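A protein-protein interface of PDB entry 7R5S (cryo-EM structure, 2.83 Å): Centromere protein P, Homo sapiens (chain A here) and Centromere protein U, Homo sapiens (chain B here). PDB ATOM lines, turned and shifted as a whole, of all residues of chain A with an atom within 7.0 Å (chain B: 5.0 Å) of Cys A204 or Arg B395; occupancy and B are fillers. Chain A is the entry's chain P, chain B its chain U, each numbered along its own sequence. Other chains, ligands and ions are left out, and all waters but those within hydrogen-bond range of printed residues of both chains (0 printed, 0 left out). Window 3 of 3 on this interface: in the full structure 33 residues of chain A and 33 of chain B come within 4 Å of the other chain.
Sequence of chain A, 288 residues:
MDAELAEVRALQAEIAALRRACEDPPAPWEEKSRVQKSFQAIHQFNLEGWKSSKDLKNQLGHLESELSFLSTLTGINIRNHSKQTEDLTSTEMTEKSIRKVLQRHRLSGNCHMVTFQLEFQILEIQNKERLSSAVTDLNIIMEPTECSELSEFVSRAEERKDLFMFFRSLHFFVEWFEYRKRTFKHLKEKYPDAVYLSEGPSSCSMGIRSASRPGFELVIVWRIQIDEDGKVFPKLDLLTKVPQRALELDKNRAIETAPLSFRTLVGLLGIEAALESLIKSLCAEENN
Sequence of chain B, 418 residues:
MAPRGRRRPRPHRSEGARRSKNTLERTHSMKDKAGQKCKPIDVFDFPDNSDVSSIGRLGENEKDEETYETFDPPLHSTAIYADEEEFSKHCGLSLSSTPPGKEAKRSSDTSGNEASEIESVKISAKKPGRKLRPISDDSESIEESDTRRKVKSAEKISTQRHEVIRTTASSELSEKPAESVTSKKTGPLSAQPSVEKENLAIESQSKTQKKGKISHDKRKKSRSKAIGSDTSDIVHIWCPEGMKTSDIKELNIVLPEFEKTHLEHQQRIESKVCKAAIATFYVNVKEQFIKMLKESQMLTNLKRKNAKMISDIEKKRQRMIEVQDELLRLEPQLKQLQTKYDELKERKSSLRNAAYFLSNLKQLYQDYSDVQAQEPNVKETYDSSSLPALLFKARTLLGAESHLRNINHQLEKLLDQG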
ATOM      1  N   GLU A 146       7.752 -14.312  19.052  1.00  0.00           N
ATOM      2  CA  GLU A 146       8.632 -13.176  18.819  1.00  0.00           C
ATOM      3  C   GLU A 146       9.747 -13.072  19.852  1.00  0.00           C
ATOM      4  O   GLU A 146      10.504 -12.096  19.835  1.00  0.00           O
ATOM      5  CB  GLU A 146       7.826 -11.876  18.799  1.00  0.00           C
ATOM      6  N   PHE A 177       7.501 -14.910  33.351  1.00  0.00           N
ATOM      7  CA  PHE A 177       6.603 -14.358  32.342  1.00  0.00           C
ATOM      8  C   PHE A 177       5.195 -14.185  32.900  1.00  0.00           C
ATOM      9  O   PHE A 177       4.569 -13.134  32.721  1.00  0.00           O
ATOM     10  CB  PHE A 177       6.590 -15.258  31.106  1.00  0.00           C
ATOM     11  CG  PHE A 177       5.781 -14.713  29.964  1.00  0.00           C
ATOM     12  CD1 PHE A 177       6.314 -13.757  29.115  1.00  0.00           C
ATOM     13  CD2 PHE A 177       4.490 -15.160  29.737  1.00  0.00           C
ATOM     14  CE1 PHE A 177       5.572 -13.254  28.063  1.00  0.00           C
ATOM     15  CE2 PHE A 177       3.745 -14.661  28.686  1.00  0.00           C
ATOM     16  CZ  PHE A 177       4.286 -13.707  27.848  1.00  0.00           C
ATOM     17  N   ARG A 180       5.188 -11.226  35.347  1.00  0.00           N
ATOM     18  CA  ARG A 180       5.088  -9.939  34.665  1.00  0.00           C
ATOM     19  C   ARG A 180       3.694  -9.724  34.090  1.00  0.00           C
ATOM     20  O   ARG A 180       3.162  -8.607  34.131  1.00  0.00           O
ATOM     21  CB  ARG A 180       6.142  -9.845  33.561  1.00  0.00           C
ATOM     22  CG  ARG A 180       6.129  -8.523  32.809  1.00  0.00           C
ATOM     23  CD  ARG A 180       7.198  -8.485  31.729  1.00  0.00           C
ATOM     24  NE  ARG A 180       6.976  -9.498  30.702  1.00  0.00           N
ATOM     25  CZ  ARG A 180       7.744  -9.650  29.627  1.00  0.00           C
ATOM     26  NH1 ARG A 180       8.787  -8.855  29.437  1.00  0.00           N
ATOM     27  NH2 ARG A 180       7.468 -10.598  28.742  1.00  0.00           N
ATOM     28  N   PHE A 184       1.382  -6.579  35.237  1.00  0.00           N
ATOM     29  CA  PHE A 184       1.037  -5.480  34.340  1.00  0.00           C
ATOM     30  C   PHE A 184      -0.471  -5.278  34.254  1.00  0.00           C
ATOM     31  O   PHE A 184      -0.950  -4.138  34.246  1.00  0.00           O
ATOM     32  CB  PHE A 184       1.623  -5.730  32.950  1.00  0.00           C
ATOM     33  CG  PHE A 184       2.971  -5.103  32.740  1.00  0.00           C
ATOM     34  CD1 PHE A 184       3.619  -4.453  33.777  1.00  0.00           C
ATOM     35  CD2 PHE A 184       3.589  -5.158  31.501  1.00  0.00           C
ATOM     36  CE1 PHE A 184       4.859  -3.874  33.584  1.00  0.00           C
ATOM     37  CE2 PHE A 184       4.829  -4.581  31.302  1.00  0.00           C
ATOM     38  CZ  PHE A 184       5.465  -3.939  32.345  1.00  0.00           C
ATOM     39  N   GLU A 199       1.078  -2.226  23.791  1.00  0.00           N
ATOM     40  CA  GLU A 199       1.285  -3.512  23.139  1.00  0.00           C
ATOM     41  C   GLU A 199       0.522  -4.661  23.779  1.00  0.00           C
ATOM     42  O   GLU A 199       0.187  -5.622  23.083  1.00  0.00           O
ATOM     43  CB  GLU A 199       2.779  -3.861  23.112  1.00  0.00           C
ATOM     44  CG  GLU A 199       3.160  -4.868  22.038  1.00  0.00           C
ATOM     45  CD  GLU A 199       2.892  -4.359  20.635  1.00  0.00           C
ATOM     46  OE1 GLU A 199       2.985  -3.134  20.415  1.00  0.00           O
ATOM     47  OE2 GLU A 199       2.584  -5.188  19.752  1.00  0.00           O
ATOM     48  N   GLY A 200       0.236  -4.593  25.076  1.00  0.00           N
ATOM     49  CA  GLY A 200      -0.517  -5.632  25.737  1.00  0.00           C
ATOM     50  C   GLY A 200       0.155  -6.140  26.996  1.00  0.00           C
ATOM     51  O   GLY A 200       1.326  -5.852  27.264  1.00  0.00           O
ATOM     52  N   PRO A 201      -0.583  -6.913  27.798  1.00  0.00           N
ATOM     53  CA  PRO A 201      -0.006  -7.431  29.050  1.00  0.00           C
ATOM     54  C   PRO A 201       1.055  -8.495  28.838  1.00  0.00           C
ATOM     55  O   PRO A 201       1.845  -8.746  29.756  1.00  0.00           O
ATOM     56  CB  PRO A 201      -1.225  -8.001  29.787  1.00  0.00           C
ATOM     57  CG  PRO A 201      -2.183  -8.355  28.698  1.00  0.00           C
ATOM     58  CD  PRO A 201      -1.985  -7.328  27.617  1.00  0.00           C
ATOM     59  N   SER A 202       1.102  -9.126  27.663  1.00  0.00           N
ATOM     60  CA  SER A 202       2.104 -10.138  27.353  1.00  0.00           C
ATOM     61  C   SER A 202       3.324  -9.556  26.650  1.00  0.00           C
ATOM     62  O   SER A 202       3.977 -10.254  25.863  1.00  0.00           O
ATOM     63  CB  SER A 202       1.483 -11.251  26.509  1.00  0.00           C
ATOM     64  OG  SER A 202       0.971 -10.741  25.290  1.00  0.00           O
ATOM     65  N   SER A 203       3.648  -8.295  26.912  1.00  0.00           N
ATOM     66  CA  SER A 203       4.752  -7.604  26.263  1.00  0.00           C
ATOM     67  C   SER A 203       5.795  -7.212  27.309  1.00  0.00           C
ATOM     68  O   SER A 203       5.695  -7.573  28.485  1.00  0.00           O
ATOM     69  CB  SER A 203       4.235  -6.389  25.490  1.00  0.00           C
ATOM     70  OG  SER A 203       3.238  -6.774  24.562  1.00  0.00           O
ATOM     71  N   CYS A 204       6.804  -6.464  26.868  1.00  0.00           N
ATOM     72  CA  CYS A 204       7.912  -6.052  27.722  1.00  0.00           C
ATOM     73  C   CYS A 204       7.856  -4.589  28.127  1.00  0.00           C
ATOM     74  O   CYS A 204       8.224  -4.253  29.253  1.00  0.00           O
ATOM     75  CB  CYS A 204       9.247  -6.326  27.019  1.00  0.00           C
ATOM     76  SG  CYS A 204       9.300  -7.881  26.099  1.00  0.00           S
ATOM     77  N   SER A 205       7.407  -3.708  27.238  1.00  0.00           N
ATOM     78  CA  SER A 205       7.378  -2.286  27.534  1.00  0.00           C
ATOM     79  C   SER A 205       6.106  -1.919  28.298  1.00  0.00           C
ATOM     80  O   SER A 205       5.167  -2.710  28.423  1.00  0.00           O
ATOM     81  CB  SER A 205       7.479  -1.470  26.248  1.00  0.00           C
ATOM     82  OG  SER A 205       6.200  -1.265  25.671  1.00  0.00           O
ATOM     83  N   MET A 206       6.089  -0.693  28.815  1.00  0.00           N
ATOM     84  CA  MET A 206       4.932  -0.165  29.522  1.00  0.00           C
ATOM     85  C   MET A 206       4.969   1.352  29.421  1.00  0.00           C
ATOM     86  O   MET A 206       6.019   1.959  29.625  1.00  0.00           O
ATOM     87  CB  MET A 206       4.925  -0.610  30.989  1.00  0.00           C
ATOM     88  CG  MET A 206       3.918   0.113  31.866  1.00  0.00           C
ATOM     89  SD  MET A 206       4.033  -0.408  33.589  1.00  0.00           S
ATOM     90  CE  MET A 206       2.908   0.742  34.374  1.00  0.00           C
ATOM     91  N   ILE A 220       8.375   2.445  31.156  1.00  0.00           N
ATOM     92  CA  ILE A 220       9.073   1.512  32.030  1.00  0.00           C
ATOM     93  C   ILE A 220       9.308   0.227  31.251  1.00  0.00           C
ATOM     94  O   ILE A 220       8.413  -0.255  30.543  1.00  0.00           O
ATOM     95  CB  ILE A 220       8.276   1.245  33.322  1.00  0.00           C
ATOM     96  CG1 ILE A 220       8.006   2.559  34.056  1.00  0.00           C
ATOM     97  CG2 ILE A 220       9.026   0.278  34.225  1.00  0.00           C
ATOM     98  CD1 ILE A 220       7.155   2.405  35.294  1.00  0.00           C
ATOM     99  N   VAL A 221      10.513  -0.323  31.375  1.00  0.00           N
ATOM    100  CA  VAL A 221      10.942  -1.483  30.604  1.00  0.00           C
ATOM    101  C   VAL A 221      11.135  -2.655  31.556  1.00  0.00           C
ATOM    102  O   VAL A 221      11.805  -2.522  32.584  1.00  0.00           O
ATOM    103  CB  VAL A 221      12.239  -1.193  29.827  1.00  0.00           C
ATOM    104  CG1 VAL A 221      12.696  -2.430  29.074  1.00  0.00           C
ATOM    105  CG2 VAL A 221      12.040  -0.019  28.881  1.00  0.00           C
ATOM    106  N   TRP A 222      10.547  -3.799  31.208  1.00  0.00           N
ATOM    107  CA  TRP A 222      10.690  -5.031  31.976  1.00  0.00           C
ATOM    108  C   TRP A 222      11.075  -6.144  31.010  1.00  0.00           C
ATOM    109  O   TRP A 222      10.265  -6.544  30.167  1.00  0.00           O
ATOM    110  CB  TRP A 222       9.400  -5.373  32.724  1.00  0.00           C
ATOM    111  CG  TRP A 222       9.569  -6.405  33.801  1.00  0.00           C
ATOM    112  CD1 TRP A 222      10.602  -7.289  33.939  1.00  0.00           C
ATOM    113  CD2 TRP A 222       8.679  -6.658  34.894  1.00  0.00           C
ATOM    114  NE1 TRP A 222      10.407  -8.075  35.047  1.00  0.00           N
ATOM    115  CE2 TRP A 222       9.234  -7.708  35.652  1.00  0.00           C
ATOM    116  CE3 TRP A 222       7.466  -6.098  35.305  1.00  0.00           C
ATOM    117  CZ2 TRP A 222       8.618  -8.209  36.796  1.00  0.00           C
ATOM    118  CZ3 TRP A 222       6.856  -6.597  36.442  1.00  0.00           C
ATOM    119  CH2 TRP A 222       7.432  -7.641  37.174  1.00  0.00           C
ATOM    120  N   ARG A 223      12.302  -6.639  31.132  1.00  0.00           N
ATOM    121  CA  ARG A 223      12.817  -7.687  30.265  1.00  0.00           C
ATOM    122  C   ARG A 223      13.212  -8.903  31.091  1.00  0.00           C
ATOM    123  O   ARG A 223      13.446  -8.813  32.299  1.00  0.00           O
ATOM    124  CB  ARG A 223      14.022  -7.197  29.451  1.00  0.00           C
ATOM    125  CG  ARG A 223      13.679  -6.170  28.387  1.00  0.00           C
ATOM    126  CD  ARG A 223      14.843  -5.223  28.143  1.00  0.00           C
ATOM    127  NE  ARG A 223      16.088  -5.939  27.884  1.00  0.00           N
ATOM    128  CZ  ARG A 223      17.273  -5.351  27.754  1.00  0.00           C
ATOM    129  NH1 ARG A 223      17.376  -4.034  27.861  1.00  0.00           N
ATOM    130  NH2 ARG A 223      18.356  -6.080  27.521  1.00  0.00           N
ATOM    131  N   ILE A 224      13.279 -10.048  30.419  1.00  0.00           N
ATOM    132  CA  ILE A 224      13.689 -11.308  31.027  1.00  0.00           C
ATOM    133  C   ILE A 224      14.960 -11.773  30.333  1.00  0.00           C
ATOM    134  O   ILE A 224      14.998 -11.875  29.101  1.00  0.00           O
ATOM    135  CB  ILE A 224      12.583 -12.375  30.924  1.00  0.00           C
ATOM    136  CG1 ILE A 224      11.290 -11.862  31.561  1.00  0.00           C
ATOM    137  CG2 ILE A 224      13.028 -13.667  31.585  1.00  0.00           C
ATOM    138  CD1 ILE A 224      10.139 -12.838  31.477  1.00  0.00           C
ATOM    139  N   LEU B 391      13.061   5.412  20.731  1.00  0.00           N
ATOM    140  CA  LEU B 391      13.411   4.156  20.080  1.00  0.00           C
ATOM    141  C   LEU B 391      12.559   3.008  20.604  1.00  0.00           C
ATOM    142  O   LEU B 391      12.168   2.120  19.841  1.00  0.00           O
ATOM    143  CB  LEU B 391      14.896   3.855  20.276  1.00  0.00           C
ATOM    144  CG  LEU B 391      15.814   4.202  19.101  1.00  0.00           C
ATOM    145  CD1 LEU B 391      17.244   3.770  19.388  1.00  0.00           C
ATOM    146  CD2 LEU B 391      15.305   3.565  17.816  1.00  0.00           C
ATOM    147  N   PHE B 392      12.246   3.011  21.900  1.00  0.00           N
ATOM    148  CA  PHE B 392      11.361   1.977  22.422  1.00  0.00           C
ATOM    149  C   PHE B 392       9.923   2.159  21.954  1.00  0.00           C
ATOM    150  O   PHE B 392       9.155   1.191  21.958  1.00  0.00           O
ATOM    151  CB  PHE B 392      11.419   1.937  23.948  1.00  0.00           C
ATOM    152  CG  PHE B 392      12.089   0.709  24.488  1.00  0.00           C
ATOM    153  CD1 PHE B 392      13.437   0.486  24.266  1.00  0.00           C
ATOM    154  CD2 PHE B 392      11.365  -0.240  25.191  1.00  0.00           C
ATOM    155  CE1 PHE B 392      14.057  -0.647  24.754  1.00  0.00           C
ATOM    156  CE2 PHE B 392      11.979  -1.378  25.678  1.00  0.00           C
ATOM    157  CZ  PHE B 392      13.327  -1.581  25.461  1.00  0.00           C
ATOM    158  N   LYS B 393       9.540   3.375  21.561  1.00  0.00           N
ATOM    159  CA  LYS B 393       8.234   3.578  20.942  1.00  0.00           C
ATOM    160  C   LYS B 393       8.239   3.134  19.483  1.00  0.00           C
ATOM    161  O   LYS B 393       7.241   2.596  18.991  1.00  0.00           O
ATOM    162  CB  LYS B 393       7.821   5.045  21.051  1.00  0.00           C
ATOM    163  CG  LYS B 393       7.181   5.416  22.379  1.00  0.00           C
ATOM    164  CD  LYS B 393       6.572   6.806  22.324  1.00  0.00           C
ATOM    165  CE  LYS B 393       5.725   7.090  23.555  1.00  0.00           C
ATOM    166  NZ  LYS B 393       5.077   8.428  23.479  1.00  0.00           N
ATOM    167  N   ALA B 394       9.350   3.360  18.777  1.00  0.00           N
ATOM    168  CA  ALA B 394       9.502   2.864  17.413  1.00  0.00           C
ATOM    169  C   ALA B 394       9.802   1.371  17.362  1.00  0.00           C
ATOM    170  O   ALA B 394       9.865   0.805  16.264  1.00  0.00           O
ATOM    171  CB  ALA B 394      10.607   3.638  16.692  1.00  0.00           C
ATOM    172  N   ARG B 395      10.035   0.742  18.514  1.00  0.00           N
ATOM    173  CA  ARG B 395      10.200  -0.707  18.570  1.00  0.00           C
ATOM    174  C   ARG B 395       9.038  -1.420  17.889  1.00  0.00           C
ATOM    175  O   ARG B 395       9.234  -2.201  16.952  1.00  0.00           O
ATOM    176  CB  ARG B 395      10.331  -1.159  20.026  1.00  0.00           C
ATOM    177  CG  ARG B 395      10.154  -2.651  20.226  1.00  0.00           C
ATOM    178  CD  ARG B 395       9.938  -2.984  21.689  1.00  0.00           C
ATOM    179  NE  ARG B 395       9.642  -4.399  21.885  1.00  0.00           N
ATOM    180  CZ  ARG B 395       9.372  -4.949  23.064  1.00  0.00           C
ATOM    181  NH1 ARG B 395       9.357  -4.203  24.159  1.00  0.00           N
ATOM    182  NH2 ARG B 395       9.115  -6.248  23.147  1.00  0.00           N
ATOM    183  N   THR B 396       7.814  -1.158  18.353  1.00  0.00           N
ATOM    184  CA  THR B 396       6.643  -1.758  17.722  1.00  0.00           C
ATOM    185  C   THR B 396       6.462  -1.262  16.293  1.00  0.00           C
ATOM    186  O   THR B 396       5.969  -2.006  15.439  1.00  0.00           O
ATOM    187  CB  THR B 396       5.388  -1.472  18.548  1.00  0.00           C
ATOM    188  OG1 THR B 396       4.226  -1.875  17.812  1.00  0.00           O
ATOM    189  CG2 THR B 396       5.283   0.008  18.879  1.00  0.00           C
ATOM    190  N   LEU B 397       6.875  -0.024  16.012  1.00  0.00           N
ATOM    191  CA  LEU B 397       6.781   0.503  14.654  1.00  0.00           C
ATOM    192  C   LEU B 397       7.550  -0.381  13.679  1.00  0.00           C
ATOM    193  O   LEU B 397       7.028  -0.770  12.628  1.00  0.00           O
ATOM    194  CB  LEU B 397       7.318   1.935  14.624  1.00  0.00           C
ATOM    195  CG  LEU B 397       7.158   2.850  13.404  1.00  0.00           C
ATOM    196  CD1 LEU B 397       7.466   4.278  13.834  1.00  0.00           C
ATOM    197  CD2 LEU B 397       7.998   2.455  12.189  1.00  0.00           C
ATOM    198  N   LEU B 398       8.796  -0.705  14.016  1.00  0.00           N
ATOM    199  CA  LEU B 398       9.635  -1.514  13.140  1.00  0.00           C
ATOM    200  C   LEU B 398       9.427  -3.013  13.333  1.00  0.00           C
ATOM    201  O   LEU B 398       9.910  -3.797  12.508  1.00  0.00           O
ATOM    202  CB  LEU B 398      11.114  -1.163  13.343  1.00  0.00           C
ATOM    203  CG  LEU B 398      11.617   0.118  12.658  1.00  0.00           C
ATOM    204  CD1 LEU B 398      11.217   1.371  13.424  1.00  0.00           C
ATOM    205  CD2 LEU B 398      13.122   0.087  12.434  1.00  0.00           C
ATOM    206  N   GLY B 399       8.729  -3.429  14.386  1.00  0.00           N
ATOM    207  CA  GLY B 399       8.379  -4.819  14.588  1.00  0.00           C
ATOM    208  C   GLY B 399       6.947  -5.173  14.255  1.00  0.00           C
ATOM    209  O   GLY B 399       6.496  -6.268  14.617  1.00  0.00           O
ATOM    210  N   ALA B 400       6.201  -4.261  13.626  1.00  0.00           N
ATOM    211  CA  ALA B 400       4.866  -4.595  13.139  1.00  0.00           C
ATOM    212  C   ALA B 400       4.867  -5.840  12.261  1.00  0.00           C
ATOM    213  O   ALA B 400       3.870  -6.564  12.218  1.00  0.00           O
ATOM    214  CB  ALA B 400       4.278  -3.409  12.374  1.00  0.00           C
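The side-chain carboxylate (OE1) of Glu A199 sits at hydrogen-bond distance from the side-chain hydroxyl (OG1) of Thr B396, at 3.1 Å. The side-chain sulfur of Cys A204 sits at hydrogen-bond distance from the guanidinium group of Arg B395, 3.4 Å away.
The backbone NH (N) of Trp A222 lies within hydrogen-bond range of the backbone carbonyl oxygen (O) of Cys A204 (3.1 Å). NH1 of Arg A180 lies close to SG of Cys A204 (3.5 Å).
Among the printed residues, merely in contact across the chains: Val A221 with Phe B392 (3.5 Å) and Ser A205 with Arg B395 (3.7 Å).
Printed residues of chain B within 4 Å of Cys A204: Arg B395 (3.4 Å). Of the printed residues of chain A, Thr B396 touches Glu A199. Printed residues of chain B within 4 Å of Ser A205: Arg B395. Printed residues of chain B within 4 Å of Val A221: Phe B392. Printed residues of chain A within 4 Å of Phe B392: Val A221 (3.5 Å). The nearest residue of chain A that does not touch Arg B395 is Ser A203 (5.4 Å). The nearest printed residue of chain A that does not touch Thr B396 is Ser A205 (7.0 Å).
Printed residues of chain B that touch a printed residue of chain A: Phe B392, Arg B395 and Thr B396. Hydrophobic or aromatic side chains of chain B that line the printed part of chain A: Phe B392. Hydrophobic or aromatic side chains of chain A that line the printed part of chain B: Val A221. Among the printed residues, 4 pairs touch across the chains. Among the printed residues, no Asp or Glu carboxylate lies within 4 Å of a Lys or Arg side-chain nitrogen of the other chain.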
